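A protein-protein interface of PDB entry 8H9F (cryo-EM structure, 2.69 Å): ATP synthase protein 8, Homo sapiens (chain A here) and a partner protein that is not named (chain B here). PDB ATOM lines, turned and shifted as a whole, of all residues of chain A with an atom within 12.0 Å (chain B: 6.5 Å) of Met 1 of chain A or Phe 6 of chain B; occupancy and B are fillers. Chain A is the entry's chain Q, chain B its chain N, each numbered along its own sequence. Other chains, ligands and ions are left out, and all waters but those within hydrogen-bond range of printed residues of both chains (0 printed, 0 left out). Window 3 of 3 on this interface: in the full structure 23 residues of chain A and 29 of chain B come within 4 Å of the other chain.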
ATOM      1  N   MET A   1     -31.887 -24.158  27.635  1.00  0.00           N
ATOM      2  CA  MET A   1     -31.709 -23.219  28.735  1.00  0.00           C
ATOM      3  C   MET A   1     -30.231 -23.005  29.026  1.00  0.00           C
ATOM      4  O   MET A   1     -29.571 -23.887  29.568  1.00  0.00           O
ATOM      5  CB  MET A   1     -32.419 -23.720  29.992  1.00  0.00           C
ATOM      6  CG  MET A   1     -33.927 -23.815  29.865  1.00  0.00           C
ATOM      7  SD  MET A   1     -34.714 -22.229  29.551  1.00  0.00           S
ATOM      8  CE  MET A   1     -34.470 -21.424  31.127  1.00  0.00           C
ATOM      9  N   PRO A   2     -29.708 -21.832  28.665  1.00  0.00           N
ATOM     10  CA  PRO A   2     -28.292 -21.548  28.944  1.00  0.00           C
ATOM     11  C   PRO A   2     -27.963 -21.490  30.424  1.00  0.00           C
ATOM     12  O   PRO A   2     -26.786 -21.598  30.784  1.00  0.00           O
ATOM     13  CB  PRO A   2     -28.063 -20.191  28.265  1.00  0.00           C
ATOM     14  CG  PRO A   2     -29.419 -19.609  28.091  1.00  0.00           C
ATOM     15  CD  PRO A   2     -30.352 -20.752  27.902  1.00  0.00           C
ATOM     16  N   GLN A   3     -28.959 -21.321  31.294  1.00  0.00           N
ATOM     17  CA  GLN A   3     -28.721 -21.383  32.729  1.00  0.00           C
ATOM     18  C   GLN A   3     -28.433 -22.796  33.210  1.00  0.00           C
ATOM     19  O   GLN A   3     -27.989 -22.965  34.350  1.00  0.00           O
ATOM     20  CB  GLN A   3     -29.922 -20.821  33.485  1.00  0.00           C
ATOM     21  CG  GLN A   3     -30.115 -19.332  33.324  1.00  0.00           C
ATOM     22  CD  GLN A   3     -31.045 -18.981  32.187  1.00  0.00           C
ATOM     23  OE1 GLN A   3     -30.978 -19.569  31.112  1.00  0.00           O
ATOM     24  NE2 GLN A   3     -31.920 -18.016  32.419  1.00  0.00           N
ATOM     25  N   LEU A   4     -28.680 -23.807  32.381  1.00  0.00           N
ATOM     26  CA  LEU A   4     -28.421 -25.189  32.753  1.00  0.00           C
ATOM     27  C   LEU A   4     -27.038 -25.662  32.339  1.00  0.00           C
ATOM     28  O   LEU A   4     -26.565 -26.679  32.857  1.00  0.00           O
ATOM     29  CB  LEU A   4     -29.482 -26.106  32.137  1.00  0.00           C
ATOM     30  CG  LEU A   4     -30.667 -26.496  33.024  1.00  0.00           C
ATOM     31  CD1 LEU A   4     -30.202 -27.376  34.166  1.00  0.00           C
ATOM     32  CD2 LEU A   4     -31.383 -25.272  33.556  1.00  0.00           C
ATOM     33  N   ASN A   5     -26.381 -24.955  31.424  1.00  0.00           N
ATOM     34  CA  ASN A   5     -25.024 -25.289  31.008  1.00  0.00           C
ATOM     35  C   ASN A   5     -24.066 -25.019  32.160  1.00  0.00           C
ATOM     36  O   ASN A   5     -23.750 -23.863  32.455  1.00  0.00           O
ATOM     37  CB  ASN A   5     -24.645 -24.475  29.774  1.00  0.00           C
ATOM     38  CG  ASN A   5     -23.199 -24.661  29.372  1.00  0.00           C
ATOM     39  OD1 ASN A   5     -22.575 -25.670  29.696  1.00  0.00           O
ATOM     40  ND2 ASN A   5     -22.656 -23.685  28.657  1.00  0.00           N
ATOM     41  N   THR A   6     -23.594 -26.082  32.808  1.00  0.00           N
ATOM     42  CA  THR A   6     -22.753 -25.961  33.992  1.00  0.00           C
ATOM     43  C   THR A   6     -21.290 -25.687  33.671  1.00  0.00           C
ATOM     44  O   THR A   6     -20.475 -25.624  34.597  1.00  0.00           O
ATOM     45  CB  THR A   6     -22.855 -27.228  34.842  1.00  0.00           C
ATOM     46  OG1 THR A   6     -22.427 -28.356  34.072  1.00  0.00           O
ATOM     47  CG2 THR A   6     -24.282 -27.447  35.297  1.00  0.00           C
ATOM     48  N   THR A   7     -20.933 -25.527  32.397  1.00  0.00           N
ATOM     49  CA  THR A   7     -19.541 -25.262  32.053  1.00  0.00           C
ATOM     50  C   THR A   7     -19.134 -23.841  32.417  1.00  0.00           C
ATOM     51  O   THR A   7     -17.995 -23.611  32.837  1.00  0.00           O
ATOM     52  CB  THR A   7     -19.317 -25.518  30.564  1.00  0.00           C
ATOM     53  OG1 THR A   7     -19.649 -26.878  30.263  1.00  0.00           O
ATOM     54  CG2 THR A   7     -17.871 -25.269  30.185  1.00  0.00           C
ATOM     55  N   VAL A   8     -20.045 -22.885  32.284  1.00  0.00           N
ATOM     56  CA  VAL A   8     -19.756 -21.491  32.582  1.00  0.00           C
ATOM     57  C   VAL A   8     -20.195 -21.120  33.999  1.00  0.00           C
ATOM     58  O   VAL A   8     -20.343 -19.942  34.310  1.00  0.00           O
ATOM     59  CB  VAL A   8     -20.388 -20.554  31.544  1.00  0.00           C
ATOM     60  CG1 VAL A   8     -19.874 -20.882  30.157  1.00  0.00           C
ATOM     61  CG2 VAL A   8     -21.899 -20.659  31.589  1.00  0.00           C
ATOM     62  N   TRP A   9     -20.401 -22.114  34.867  1.00  0.00           N
ATOM     63  CA  TRP A   9     -20.884 -21.811  36.212  1.00  0.00           C
ATOM     64  C   TRP A   9     -19.827 -21.133  37.074  1.00  0.00           C
ATOM     65  O   TRP A   9     -20.153 -20.123  37.720  1.00  0.00           O
ATOM     66  CB  TRP A   9     -21.431 -23.080  36.869  1.00  0.00           C
ATOM     67  CG  TRP A   9     -22.869 -23.320  36.558  1.00  0.00           C
ATOM     68  CD1 TRP A   9     -23.523 -22.987  35.411  1.00  0.00           C
ATOM     69  CD2 TRP A   9     -23.839 -23.941  37.408  1.00  0.00           C
ATOM     70  NE1 TRP A   9     -24.840 -23.363  35.491  1.00  0.00           N
ATOM     71  CE2 TRP A   9     -25.059 -23.954  36.707  1.00  0.00           C
ATOM     72  CE3 TRP A   9     -23.794 -24.490  38.691  1.00  0.00           C
ATOM     73  CZ2 TRP A   9     -26.222 -24.491  37.246  1.00  0.00           C
ATOM     74  CZ3 TRP A   9     -24.949 -25.023  39.224  1.00  0.00           C
ATOM     75  CH2 TRP A   9     -26.148 -25.018  38.504  1.00  0.00           C
ATOM     76  N   MET A  12     -19.517 -17.482  36.706  1.00  0.00           N
ATOM     77  CA  MET A  12     -20.580 -16.723  37.352  1.00  0.00           C
ATOM     78  C   MET A  12     -20.465 -16.711  38.867  1.00  0.00           C
ATOM     79  O   MET A  12     -20.974 -15.786  39.508  1.00  0.00           O
ATOM     80  CB  MET A  12     -21.947 -17.287  36.963  1.00  0.00           C
ATOM     81  CG  MET A  12     -22.207 -17.312  35.479  1.00  0.00           C
ATOM     82  SD  MET A  12     -22.262 -15.666  34.769  1.00  0.00           S
ATOM     83  CE  MET A  12     -22.162 -16.076  33.037  1.00  0.00           C
ATOM     84  N   ASN B   4     -31.374 -18.432  20.262  1.00  0.00           N
ATOM     85  CA  ASN B   4     -32.400 -17.776  19.461  1.00  0.00           C
ATOM     86  C   ASN B   4     -33.251 -16.854  20.329  1.00  0.00           C
ATOM     87  O   ASN B   4     -33.255 -15.637  20.143  1.00  0.00           O
ATOM     88  CB  ASN B   4     -33.278 -18.817  18.763  1.00  0.00           C
ATOM     89  CG  ASN B   4     -33.657 -19.969  19.676  1.00  0.00           C
ATOM     90  OD1 ASN B   4     -33.352 -19.955  20.868  1.00  0.00           O
ATOM     91  ND2 ASN B   4     -34.332 -20.969  19.122  1.00  0.00           N
ATOM     92  N   LEU B   5     -33.971 -17.446  21.278  1.00  0.00           N
ATOM     93  CA  LEU B   5     -34.793 -16.704  22.223  1.00  0.00           C
ATOM     94  C   LEU B   5     -34.096 -16.463  23.549  1.00  0.00           C
ATOM     95  O   LEU B   5     -34.297 -15.411  24.163  1.00  0.00           O
ATOM     96  CB  LEU B   5     -36.107 -17.450  22.474  1.00  0.00           C
ATOM     97  CG  LEU B   5     -37.109 -16.815  23.436  1.00  0.00           C
ATOM     98  CD1 LEU B   5     -37.730 -15.581  22.811  1.00  0.00           C
ATOM     99  CD2 LEU B   5     -38.174 -17.818  23.829  1.00  0.00           C
ATOM    100  N   PHE B   6     -33.280 -17.413  24.003  1.00  0.00           N
ATOM    101  CA  PHE B   6     -32.514 -17.282  25.231  1.00  0.00           C
ATOM    102  C   PHE B   6     -31.101 -16.783  24.978  1.00  0.00           C
ATOM    103  O   PHE B   6     -30.211 -17.019  25.799  1.00  0.00           O
ATOM    104  CB  PHE B   6     -32.474 -18.619  25.969  1.00  0.00           C
ATOM    105  CG  PHE B   6     -33.814 -19.086  26.446  1.00  0.00           C
ATOM    106  CD1 PHE B   6     -34.606 -19.888  25.648  1.00  0.00           C
ATOM    107  CD2 PHE B   6     -34.284 -18.723  27.694  1.00  0.00           C
ATOM    108  CE1 PHE B   6     -35.837 -20.316  26.082  1.00  0.00           C
ATOM    109  CE2 PHE B   6     -35.518 -19.150  28.134  1.00  0.00           C
ATOM    110  CZ  PHE B   6     -36.294 -19.948  27.325  1.00  0.00           C
ATOM    111  N   ALA B   7     -30.874 -16.100  23.855  1.00  0.00           N
ATOM    112  CA  ALA B   7     -29.541 -15.605  23.540  1.00  0.00           C
ATOM    113  C   ALA B   7     -29.065 -14.550  24.527  1.00  0.00           C
ATOM    114  O   ALA B   7     -27.856 -14.342  24.656  1.00  0.00           O
ATOM    115  CB  ALA B   7     -29.514 -15.039  22.121  1.00  0.00           C
ATOM    116  N   SER B   8     -29.983 -13.879  25.222  1.00  0.00           N
ATOM    117  CA  SER B   8     -29.610 -12.855  26.186  1.00  0.00           C
ATOM    118  C   SER B   8     -29.180 -13.427  27.527  1.00  0.00           C
ATOM    119  O   SER B   8     -28.698 -12.672  28.376  1.00  0.00           O
ATOM    120  CB  SER B   8     -30.773 -11.886  26.400  1.00  0.00           C
ATOM    121  OG  SER B   8     -31.067 -11.179  25.210  1.00  0.00           O
ATOM    122  N   PHE B   9     -29.351 -14.729  27.743  1.00  0.00           N
ATOM    123  CA  PHE B   9     -28.967 -15.374  28.988  1.00  0.00           C
ATOM    124  C   PHE B   9     -27.732 -16.245  28.839  1.00  0.00           C
ATOM    125  O   PHE B   9     -27.347 -16.921  29.797  1.00  0.00           O
ATOM    126  CB  PHE B   9     -30.131 -16.206  29.532  1.00  0.00           C
ATOM    127  CG  PHE B   9     -31.446 -15.490  29.498  1.00  0.00           C
ATOM    128  CD1 PHE B   9     -32.415 -15.838  28.580  1.00  0.00           C
ATOM    129  CD2 PHE B   9     -31.708 -14.459  30.375  1.00  0.00           C
ATOM    130  CE1 PHE B   9     -33.621 -15.175  28.543  1.00  0.00           C
ATOM    131  CE2 PHE B   9     -32.914 -13.794  30.339  1.00  0.00           C
ATOM    132  CZ  PHE B   9     -33.869 -14.155  29.422  1.00  0.00           C
ATOM    133  N   ILE B  10     -27.106 -16.249  27.671  1.00  0.00           N
ATOM    134  CA  ILE B  10     -25.870 -16.989  27.463  1.00  0.00           C
ATOM    135  C   ILE B  10     -24.707 -16.148  27.965  1.00  0.00           C
ATOM    136  O   ILE B  10     -24.681 -14.927  27.776  1.00  0.00           O
ATOM    137  CB  ILE B  10     -25.700 -17.350  25.978  1.00  0.00           C
ATOM    138  CG1 ILE B  10     -26.903 -18.151  25.484  1.00  0.00           C
ATOM    139  CG2 ILE B  10     -24.425 -18.139  25.759  1.00  0.00           C
ATOM    140  CD1 ILE B  10     -26.943 -18.314  23.985  1.00  0.00           C
ATOM    141  N   THR B 165     -35.703 -13.729  34.796  1.00  0.00           N
ATOM    142  CA  THR B 165     -35.689 -14.314  33.460  1.00  0.00           C
ATOM    143  C   THR B 165     -37.044 -14.185  32.778  1.00  0.00           C
ATOM    144  O   THR B 165     -37.111 -13.878  31.584  1.00  0.00           O
ATOM    145  CB  THR B 165     -35.271 -15.780  33.534  1.00  0.00           C
ATOM    146  OG1 THR B 165     -34.051 -15.891  34.273  1.00  0.00           O
ATOM    147  CG2 THR B 165     -35.061 -16.343  32.145  1.00  0.00           C
ATOM    148  N   LEU B 169     -37.839 -12.169  29.371  1.00  0.00           N
ATOM    149  CA  LEU B 169     -38.445 -12.872  28.245  1.00  0.00           C
ATOM    150  C   LEU B 169     -39.717 -12.184  27.779  1.00  0.00           C
ATOM    151  O   LEU B 169     -39.938 -12.028  26.574  1.00  0.00           O
ATOM    152  CB  LEU B 169     -38.741 -14.321  28.621  1.00  0.00           C
ATOM    153  CG  LEU B 169     -37.623 -15.332  28.395  1.00  0.00           C
ATOM    154  CD1 LEU B 169     -37.955 -16.642  29.076  1.00  0.00           C
ATOM    155  CD2 LEU B 169     -37.413 -15.539  26.911  1.00  0.00           C
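The backbone carbonyl oxygen (O) of Gln 3 of chain A sits at hydrogen-bond distance from the indole nitrogen (NE1) of Trp 9 of chain A.
Among the printed residues, merely in contact across the chains: Met 1 of chain A with Phe 6 of chain B (3.5 Å), Pro 2 of chain A with Phe 6 of chain B (3.5 Å), Pro 2 of chain A with Phe 9 of chain B (3.7 Å), Pro 2 of chain A with Ile 10 of chain B (3.6 Å), Gln 3 of chain A with Phe 9 of chain B (3.8 Å) and Gln 3 of chain A with Thr 165 of chain B (3.5 Å).
Of chain B, only Phe 6 comes within 4 Å of Met 1 of chain A.
Of the printed residues of chain B, Pro 2 of chain A touches Phe 6 (3.5 Å), Phe 9 (3.7 Å) and Ile 10 (3.6 Å).
Of the printed residues of chain B, Gln 3 of chain A touches Phe 9 (3.8 Å) and Thr 165 (3.5 Å).
No residue of chain A comes within 4 Å of Asn 4 of chain B.
No residue of chain A comes within 4 Å of Leu 5 of chain B.
Phe 6 of chain B touches just these residues of chain A: Met 1 (3.5 Å) and Pro 2 (3.5 Å).
No residue of chain A comes within 4 Å of Ala 7 of chain B.
No residue of chain A comes within 4 Å of Ser 8 of chain B.
Phe 9 of chain B touches two residues of chain A.
Of chain A, only Pro 2 comes within 4 Å of Ile 10 of chain B.
Of the printed residues of chain A, Thr 165 of chain B touches Gln 3 (3.5 Å).
Leu 169 of chain B touches none of the printed residues of chain A.
The nearest residue of chain B that does not touch Met 1 of chain A is Thr 165 of chain B (5.2 Å).
The nearest residue of chain A that does not touch Phe 6 of chain B is Gln 3 of chain A (4.8 Å).
The nearest printed residue of chain B that does not touch Gln 3 of chain A is Phe 6 of chain B (4.8 Å).
Hydrophobic or aromatic side chains of chain B within 4 Å of the printed part of chain A: Phe 6, Phe 9 and Ile 10.
Hydrophobic or aromatic side chains of chain A that line the printed part of chain B: Met 1 and Pro 2.
Among the printed residues, 6 pairs touch across the chains.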
